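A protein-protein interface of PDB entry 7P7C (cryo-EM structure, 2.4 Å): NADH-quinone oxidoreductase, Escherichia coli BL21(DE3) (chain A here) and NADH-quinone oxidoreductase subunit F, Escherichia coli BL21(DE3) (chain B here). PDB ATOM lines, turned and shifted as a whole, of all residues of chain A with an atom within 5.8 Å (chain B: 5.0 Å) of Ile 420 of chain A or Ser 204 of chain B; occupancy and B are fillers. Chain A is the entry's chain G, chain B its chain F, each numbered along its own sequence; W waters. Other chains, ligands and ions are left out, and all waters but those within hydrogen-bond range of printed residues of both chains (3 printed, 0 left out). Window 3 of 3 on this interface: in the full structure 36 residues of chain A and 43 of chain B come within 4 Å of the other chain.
Hydrophobic or aromatic side chains of chain B within 4 Å of the printed part of chain A: Pro 199. Of the 13 printed residues of chain A, 5 touch a printed residue of chain B. Printed residues of chain A that touch a printed residue of chain B: Gln 407, Ala 416, Asn 419, Ile 420 and Gln 422. Hydrophobic or aromatic side chains of chain A within 4 Å of the printed part of chain B: Ala 416 and Ile 420. Among the printed residues, 8 pairs touch across the chains.
Water W2 lies within hydrogen-bond range of the side-chain amide oxygen of Asn 419 of chain A (2.7 Å), the side-chain amide nitrogen of Gln 422 of chain A (3.0 Å) and the guanidinium group of Arg 195 of chain B (3.4 Å). Water W1 lies within hydrogen-bond range of OG of Ser 204 of chain B (2.8 Å), ND2 of Asn 419 of chain A (2.9 Å) and O of Ala 416 of chain A (3.2 Å). Water W3 lies within hydrogen-bond range of the backbone carbonyl oxygen (O) of Ile 420 of chain A (2.9 Å) and the backbone carbonyl oxygen (O) of Gly 208 of chain B (3.1 Å).
The guanidinium group (NH1) of Arg 195 of chain B lies within hydrogen-bond range of the backbone carbonyl oxygen (O) of Gly 205 of chain B, 2.9 Å away. The backbone carbonyl oxygen of Asn 419 of chain A is in hydrogen-bond range of the side-chain amide nitrogen of Gln 422 of chain A (2.6 Å).
Printed residues of chain B within 4 Å of Ile 420 of chain A: Ser 204 (3.7 Å). Of the printed residues of chain A, Gly 205 of chain B touches Asn 419 (3.4 Å). Of the printed residues of chain A, Pro 199 of chain B touches Ala 416. Of the printed residues of chain B, Gln 422 of chain A touches Gly 208. Printed residues of chain A within 4 Å of Thr 203 of chain B: Gln 407.
Among the printed residues, pairs that only touch across the chains: Gln 407 of chain A with Thr 203 of chain B, Ala 416 of chain A with Pro 199 of chain B, Asn 419 of chain A with Gly 208 of chain B, Ile 420 of chain A with Ser 204 of chain B and Gln 422 of chain A with Gly 208 of chain B.
NH1 of Arg 195 of chain B lies within hydrogen-bond range of OD1 of Asn 419 of chain A (3.1 Å). O of Ser 204 of chain B is in hydrogen-bond range of ND2 of Asn 419 of chain A. The side-chain amide nitrogen of Asn 419 of chain A lies within hydrogen-bond range of the backbone carbonyl oxygen of Gly 205 of chain B (3.4 Å).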
ATOM      1  N   ALA A 400      -0.976 -17.933   0.570  1.00  0.00           N
ATOM      2  CA  ALA A 400      -0.647 -19.314   0.907  1.00  0.00           C
ATOM      3  C   ALA A 400      -0.072 -19.402   2.309  1.00  0.00           C
ATOM      4  O   ALA A 400      -0.360 -20.355   3.047  1.00  0.00           O
ATOM      5  CB  ALA A 400       0.337 -19.887  -0.108  1.00  0.00           C
ATOM      6  N   MET A 403      -3.197 -19.228   4.657  1.00  0.00           N
ATOM      7  CA  MET A 403      -3.959 -20.476   4.704  1.00  0.00           C
ATOM      8  C   MET A 403      -3.186 -21.592   5.391  1.00  0.00           C
ATOM      9  O   MET A 403      -3.793 -22.449   6.040  1.00  0.00           O
ATOM     10  CB  MET A 403      -4.385 -20.934   3.307  1.00  0.00           C
ATOM     11  CG  MET A 403      -4.975 -19.864   2.419  1.00  0.00           C
ATOM     12  SD  MET A 403      -4.968 -20.343   0.682  1.00  0.00           S
ATOM     13  CE  MET A 403      -5.472 -22.057   0.799  1.00  0.00           C
ATOM     14  N   ALA A 404      -1.858 -21.612   5.253  1.00  0.00           N
ATOM     15  CA  ALA A 404      -1.070 -22.589   5.995  1.00  0.00           C
ATOM     16  C   ALA A 404      -1.076 -22.289   7.488  1.00  0.00           C
ATOM     17  O   ALA A 404      -1.099 -23.211   8.309  1.00  0.00           O
ATOM     18  CB  ALA A 404       0.357 -22.622   5.459  1.00  0.00           C
ATOM     19  N   GLN A 407      -4.092 -23.681   9.278  1.00  0.00           N
ATOM     20  CA  GLN A 407      -4.069 -25.116   9.523  1.00  0.00           C
ATOM     21  C   GLN A 407      -2.973 -25.528  10.499  1.00  0.00           C
ATOM     22  O   GLN A 407      -2.621 -26.711  10.551  1.00  0.00           O
ATOM     23  CB  GLN A 407      -3.908 -25.873   8.205  1.00  0.00           C
ATOM     24  CG  GLN A 407      -5.013 -25.615   7.204  1.00  0.00           C
ATOM     25  CD  GLN A 407      -5.118 -26.711   6.168  1.00  0.00           C
ATOM     26  OE1 GLN A 407      -4.526 -27.777   6.318  1.00  0.00           O
ATOM     27  NE2 GLN A 407      -5.873 -26.455   5.109  1.00  0.00           N
ATOM     28  N   VAL A 409       0.255 -24.956  10.475  1.00  0.00           N
ATOM     29  CA  VAL A 409       1.489 -25.368   9.819  1.00  0.00           C
ATOM     30  C   VAL A 409       2.551 -24.324  10.129  1.00  0.00           C
ATOM     31  O   VAL A 409       2.289 -23.119  10.037  1.00  0.00           O
ATOM     32  CB  VAL A 409       1.283 -25.536   8.303  1.00  0.00           C
ATOM     33  CG1 VAL A 409       2.606 -25.743   7.582  1.00  0.00           C
ATOM     34  CG2 VAL A 409       0.352 -26.697   8.034  1.00  0.00           C
ATOM     35  N   ALA A 415       7.358 -26.466   1.990  1.00  0.00           N
ATOM     36  CA  ALA A 415       6.686 -27.387   1.075  1.00  0.00           C
ATOM     37  C   ALA A 415       5.221 -27.579   1.449  1.00  0.00           C
ATOM     38  O   ALA A 415       4.354 -27.620   0.571  1.00  0.00           O
ATOM     39  CB  ALA A 415       7.414 -28.729   1.048  1.00  0.00           C
ATOM     40  N   ALA A 416       4.928 -27.677   2.748  1.00  0.00           N
ATOM     41  CA  ALA A 416       3.545 -27.795   3.201  1.00  0.00           C
ATOM     42  C   ALA A 416       2.750 -26.528   2.911  1.00  0.00           C
ATOM     43  O   ALA A 416       1.569 -26.598   2.551  1.00  0.00           O
ATOM     44  CB  ALA A 416       3.513 -28.115   4.690  1.00  0.00           C
ATOM     45  N   ILE A 417       3.383 -25.362   3.071  1.00  0.00           N
ATOM     46  CA  ILE A 417       2.727 -24.092   2.774  1.00  0.00           C
ATOM     47  C   ILE A 417       2.408 -23.989   1.288  1.00  0.00           C
ATOM     48  O   ILE A 417       1.321 -23.545   0.901  1.00  0.00           O
ATOM     49  CB  ILE A 417       3.604 -22.919   3.250  1.00  0.00           C
ATOM     50  CG1 ILE A 417       3.882 -23.041   4.748  1.00  0.00           C
ATOM     51  CG2 ILE A 417       2.948 -21.586   2.933  1.00  0.00           C
ATOM     52  CD1 ILE A 417       4.861 -22.031   5.276  1.00  0.00           C
ATOM     53  N   LEU A 418       3.344 -24.408   0.432  1.00  0.00           N
ATOM     54  CA  LEU A 418       3.093 -24.382  -1.004  1.00  0.00           C
ATOM     55  C   LEU A 418       2.044 -25.407  -1.414  1.00  0.00           C
ATOM     56  O   LEU A 418       1.284 -25.167  -2.357  1.00  0.00           O
ATOM     57  CB  LEU A 418       4.392 -24.618  -1.775  1.00  0.00           C
ATOM     58  CG  LEU A 418       5.493 -23.564  -1.634  1.00  0.00           C
ATOM     59  CD1 LEU A 418       6.616 -23.818  -2.628  1.00  0.00           C
ATOM     60  CD2 LEU A 418       4.935 -22.164  -1.795  1.00  0.00           C
ATOM     61  N   ASN A 419       1.992 -26.551  -0.730  1.00  0.00           N
ATOM     62  CA  ASN A 419       0.979 -27.552  -1.042  1.00  0.00           C
ATOM     63  C   ASN A 419      -0.413 -27.084  -0.639  1.00  0.00           C
ATOM     64  O   ASN A 419      -1.386 -27.333  -1.360  1.00  0.00           O
ATOM     65  CB  ASN A 419       1.315 -28.875  -0.358  1.00  0.00           C
ATOM     66  CG  ASN A 419       0.319 -29.966  -0.689  1.00  0.00           C
ATOM     67  OD1 ASN A 419       0.045 -30.238  -1.853  1.00  0.00           O
ATOM     68  ND2 ASN A 419      -0.238 -30.589   0.339  1.00  0.00           N
ATOM     69  N   ILE A 420      -0.532 -26.419   0.511  1.00  0.00           N
ATOM     70  CA  ILE A 420      -1.839 -25.948   0.963  1.00  0.00           C
ATOM     71  C   ILE A 420      -2.332 -24.813   0.076  1.00  0.00           C
ATOM     72  O   ILE A 420      -3.437 -24.867  -0.474  1.00  0.00           O
ATOM     73  CB  ILE A 420      -1.771 -25.528   2.442  1.00  0.00           C
ATOM     74  CG1 ILE A 420      -1.684 -26.765   3.331  1.00  0.00           C
ATOM     75  CG2 ILE A 420      -2.979 -24.687   2.826  1.00  0.00           C
ATOM     76  CD1 ILE A 420      -1.225 -26.476   4.722  1.00  0.00           C
ATOM     77  N   GLY A 421      -1.521 -23.776  -0.082  1.00  0.00           N
ATOM     78  CA  GLY A 421      -1.819 -22.699  -1.002  1.00  0.00           C
ATOM     79  C   GLY A 421      -1.379 -23.038  -2.407  1.00  0.00           C
ATOM     80  O   GLY A 421      -0.302 -22.612  -2.835  1.00  0.00           O
ATOM     81  N   GLN A 422      -2.185 -23.839  -3.109  1.00  0.00           N
ATOM     82  CA  GLN A 422      -1.792 -24.381  -4.409  1.00  0.00           C
ATOM     83  C   GLN A 422      -1.548 -23.276  -5.427  1.00  0.00           C
ATOM     84  O   GLN A 422      -0.413 -23.042  -5.854  1.00  0.00           O
ATOM     85  CB  GLN A 422      -2.875 -25.334  -4.911  1.00  0.00           C
ATOM     86  CG  GLN A 422      -2.883 -26.673  -4.223  1.00  0.00           C
ATOM     87  CD  GLN A 422      -1.795 -27.584  -4.736  1.00  0.00           C
ATOM     88  OE1 GLN A 422      -1.596 -27.711  -5.941  1.00  0.00           O
ATOM     89  NE2 GLN A 422      -1.083 -28.227  -3.822  1.00  0.00           N
ATOM     90  N   ARG B 195       6.956 -36.402   0.389  1.00  0.00           N
ATOM     91  CA  ARG B 195       6.744 -35.217   1.200  1.00  0.00           C
ATOM     92  C   ARG B 195       7.025 -35.524   2.663  1.00  0.00           C
ATOM     93  O   ARG B 195       6.940 -36.669   3.111  1.00  0.00           O
ATOM     94  CB  ARG B 195       5.313 -34.696   1.051  1.00  0.00           C
ATOM     95  CG  ARG B 195       4.890 -34.440  -0.372  1.00  0.00           C
ATOM     96  CD  ARG B 195       3.428 -34.069  -0.431  1.00  0.00           C
ATOM     97  NE  ARG B 195       3.023 -33.671  -1.772  1.00  0.00           N
ATOM     98  CZ  ARG B 195       1.810 -33.242  -2.089  1.00  0.00           C
ATOM     99  NH1 ARG B 195       0.852 -33.154  -1.184  1.00  0.00           N
ATOM    100  NH2 ARG B 195       1.554 -32.897  -3.345  1.00  0.00           N
ATOM    101  N   PRO B 199       2.542 -32.102   7.754  1.00  0.00           N
ATOM    102  CA  PRO B 199       1.156 -32.586   7.757  1.00  0.00           C
ATOM    103  C   PRO B 199       0.941 -33.865   6.961  1.00  0.00           C
ATOM    104  O   PRO B 199       1.619 -34.121   5.971  1.00  0.00           O
ATOM    105  CB  PRO B 199       0.386 -31.429   7.122  1.00  0.00           C
ATOM    106  CG  PRO B 199       1.360 -30.804   6.211  1.00  0.00           C
ATOM    107  CD  PRO B 199       2.707 -30.944   6.861  1.00  0.00           C
ATOM    108  N   PHE B 200      -0.008 -34.663   7.418  1.00  0.00           N
ATOM    109  CA  PHE B 200      -0.368 -35.898   6.755  1.00  0.00           C
ATOM    110  C   PHE B 200      -1.301 -35.609   5.583  1.00  0.00           C
ATOM    111  O   PHE B 200      -1.916 -34.542   5.521  1.00  0.00           O
ATOM    112  CB  PHE B 200      -1.009 -36.846   7.761  1.00  0.00           C
ATOM    113  CG  PHE B 200      -0.027 -37.448   8.720  1.00  0.00           C
ATOM    114  CD1 PHE B 200       0.343 -36.772   9.870  1.00  0.00           C
ATOM    115  CD2 PHE B 200       0.547 -38.679   8.458  1.00  0.00           C
ATOM    116  CE1 PHE B 200       1.256 -37.317  10.746  1.00  0.00           C
ATOM    117  CE2 PHE B 200       1.461 -39.231   9.332  1.00  0.00           C
ATOM    118  CZ  PHE B 200       1.816 -38.548  10.478  1.00  0.00           C
ATOM    119  N   PRO B 201      -1.398 -36.532   4.619  1.00  0.00           N
ATOM    120  CA  PRO B 201      -2.330 -36.327   3.496  1.00  0.00           C
ATOM    121  C   PRO B 201      -3.790 -36.214   3.900  1.00  0.00           C
ATOM    122  O   PRO B 201      -4.580 -35.660   3.128  1.00  0.00           O
ATOM    123  CB  PRO B 201      -2.096 -37.565   2.624  1.00  0.00           C
ATOM    124  CG  PRO B 201      -0.702 -37.948   2.902  1.00  0.00           C
ATOM    125  CD  PRO B 201      -0.461 -37.638   4.346  1.00  0.00           C
ATOM    126  N   ALA B 202      -4.173 -36.722   5.075  1.00  0.00           N
ATOM    127  CA  ALA B 202      -5.550 -36.591   5.538  1.00  0.00           C
ATOM    128  C   ALA B 202      -5.938 -35.137   5.772  1.00  0.00           C
ATOM    129  O   ALA B 202      -7.112 -34.783   5.635  1.00  0.00           O
ATOM    130  CB  ALA B 202      -5.755 -37.400   6.814  1.00  0.00           C
ATOM    131  N   THR B 203      -4.976 -34.285   6.118  1.00  0.00           N
ATOM    132  CA  THR B 203      -5.245 -32.868   6.327  1.00  0.00           C
ATOM    133  C   THR B 203      -5.025 -32.055   5.055  1.00  0.00           C
ATOM    134  O   THR B 203      -5.888 -31.267   4.661  1.00  0.00           O
ATOM    135  CB  THR B 203      -4.366 -32.338   7.462  1.00  0.00           C
ATOM    136  OG1 THR B 203      -4.731 -32.986   8.686  1.00  0.00           O
ATOM    137  CG2 THR B 203      -4.539 -30.843   7.623  1.00  0.00           C
ATOM    138  N   SER B 204      -3.882 -32.243   4.398  1.00  0.00           N
ATOM    139  CA  SER B 204      -3.575 -31.549   3.147  1.00  0.00           C
ATOM    140  C   SER B 204      -2.785 -32.511   2.268  1.00  0.00           C
ATOM    141  O   SER B 204      -1.568 -32.643   2.420  1.00  0.00           O
ATOM    142  CB  SER B 204      -2.803 -30.262   3.401  1.00  0.00           C
ATOM    143  OG  SER B 204      -1.686 -30.492   4.236  1.00  0.00           O
ATOM    144  N   GLY B 205      -3.481 -33.179   1.355  1.00  0.00           N
ATOM    145  CA  GLY B 205      -2.849 -34.154   0.493  1.00  0.00           C
ATOM    146  C   GLY B 205      -2.823 -33.743  -0.961  1.00  0.00           C
ATOM    147  O   GLY B 205      -2.055 -32.857  -1.345  1.00  0.00           O
ATOM    148  N   ALA B 206      -3.660 -34.378  -1.776  1.00  0.00           N
ATOM    149  CA  ALA B 206      -3.684 -34.106  -3.207  1.00  0.00           C
ATOM    150  C   ALA B 206      -4.284 -32.731  -3.467  1.00  0.00           C
ATOM    151  O   ALA B 206      -5.446 -32.482  -3.131  1.00  0.00           O
ATOM    152  CB  ALA B 206      -4.474 -35.188  -3.934  1.00  0.00           C
ATOM    153  N   GLY B 208      -3.632 -30.045  -1.938  1.00  0.00           N
ATOM    154  CA  GLY B 208      -3.924 -29.420  -0.669  1.00  0.00           C
ATOM    155  C   GLY B 208      -5.197 -29.882   0.005  1.00  0.00           C
ATOM    156  O   GLY B 208      -5.460 -29.466   1.140  1.00  0.00           O
ATOM    157  N   LYS B 209      -5.984 -30.724  -0.642  1.00  0.00           N
ATOM    158  CA  LYS B 209      -7.255 -31.201  -0.129  1.00  0.00           C
ATOM    159  C   LYS B 209      -7.052 -32.429   0.742  1.00  0.00           C
ATOM    160  O   LYS B 209      -6.010 -33.084   0.672  1.00  0.00           O
ATOM    161  CB  LYS B 209      -8.192 -31.527  -1.286  1.00  0.00           C
ATOM    162  CG  LYS B 209      -8.326 -30.411  -2.298  1.00  0.00           C
ATOM    163  CD  LYS B 209      -8.841 -29.142  -1.652  1.00  0.00           C
ATOM    164  CE  LYS B 209      -9.112 -28.077  -2.695  1.00  0.00           C
ATOM    165  NZ  LYS B 209      -7.884 -27.742  -3.466  1.00  0.00           N
ATOM    166  N   PRO B 210      -8.012 -32.734   1.615  1.00  0.00           N
ATOM    167  CA  PRO B 210      -7.972 -34.013   2.339  1.00  0.00           C
ATOM    168  C   PRO B 210      -7.993 -35.205   1.390  1.00  0.00           C
ATOM    169  O   PRO B 210      -8.828 -35.301   0.484  1.00  0.00           O
ATOM    170  CB  PRO B 210      -9.225 -33.964   3.224  1.00  0.00           C
ATOM    171  CG  PRO B 210      -9.879 -32.642   2.964  1.00  0.00           C
ATOM    172  CD  PRO B 210      -8.912 -31.770   2.263  1.00  0.00           C
HETATM  173  O   HOH W   1       0.606 -29.621   2.914  1.00  0.00           O
HETATM  174  O   HOH W   2       1.583 -29.533  -3.896  1.00  0.00           O
HETATM  175  O   HOH W   3      -5.746 -26.510   0.170  1.00  0.00           O
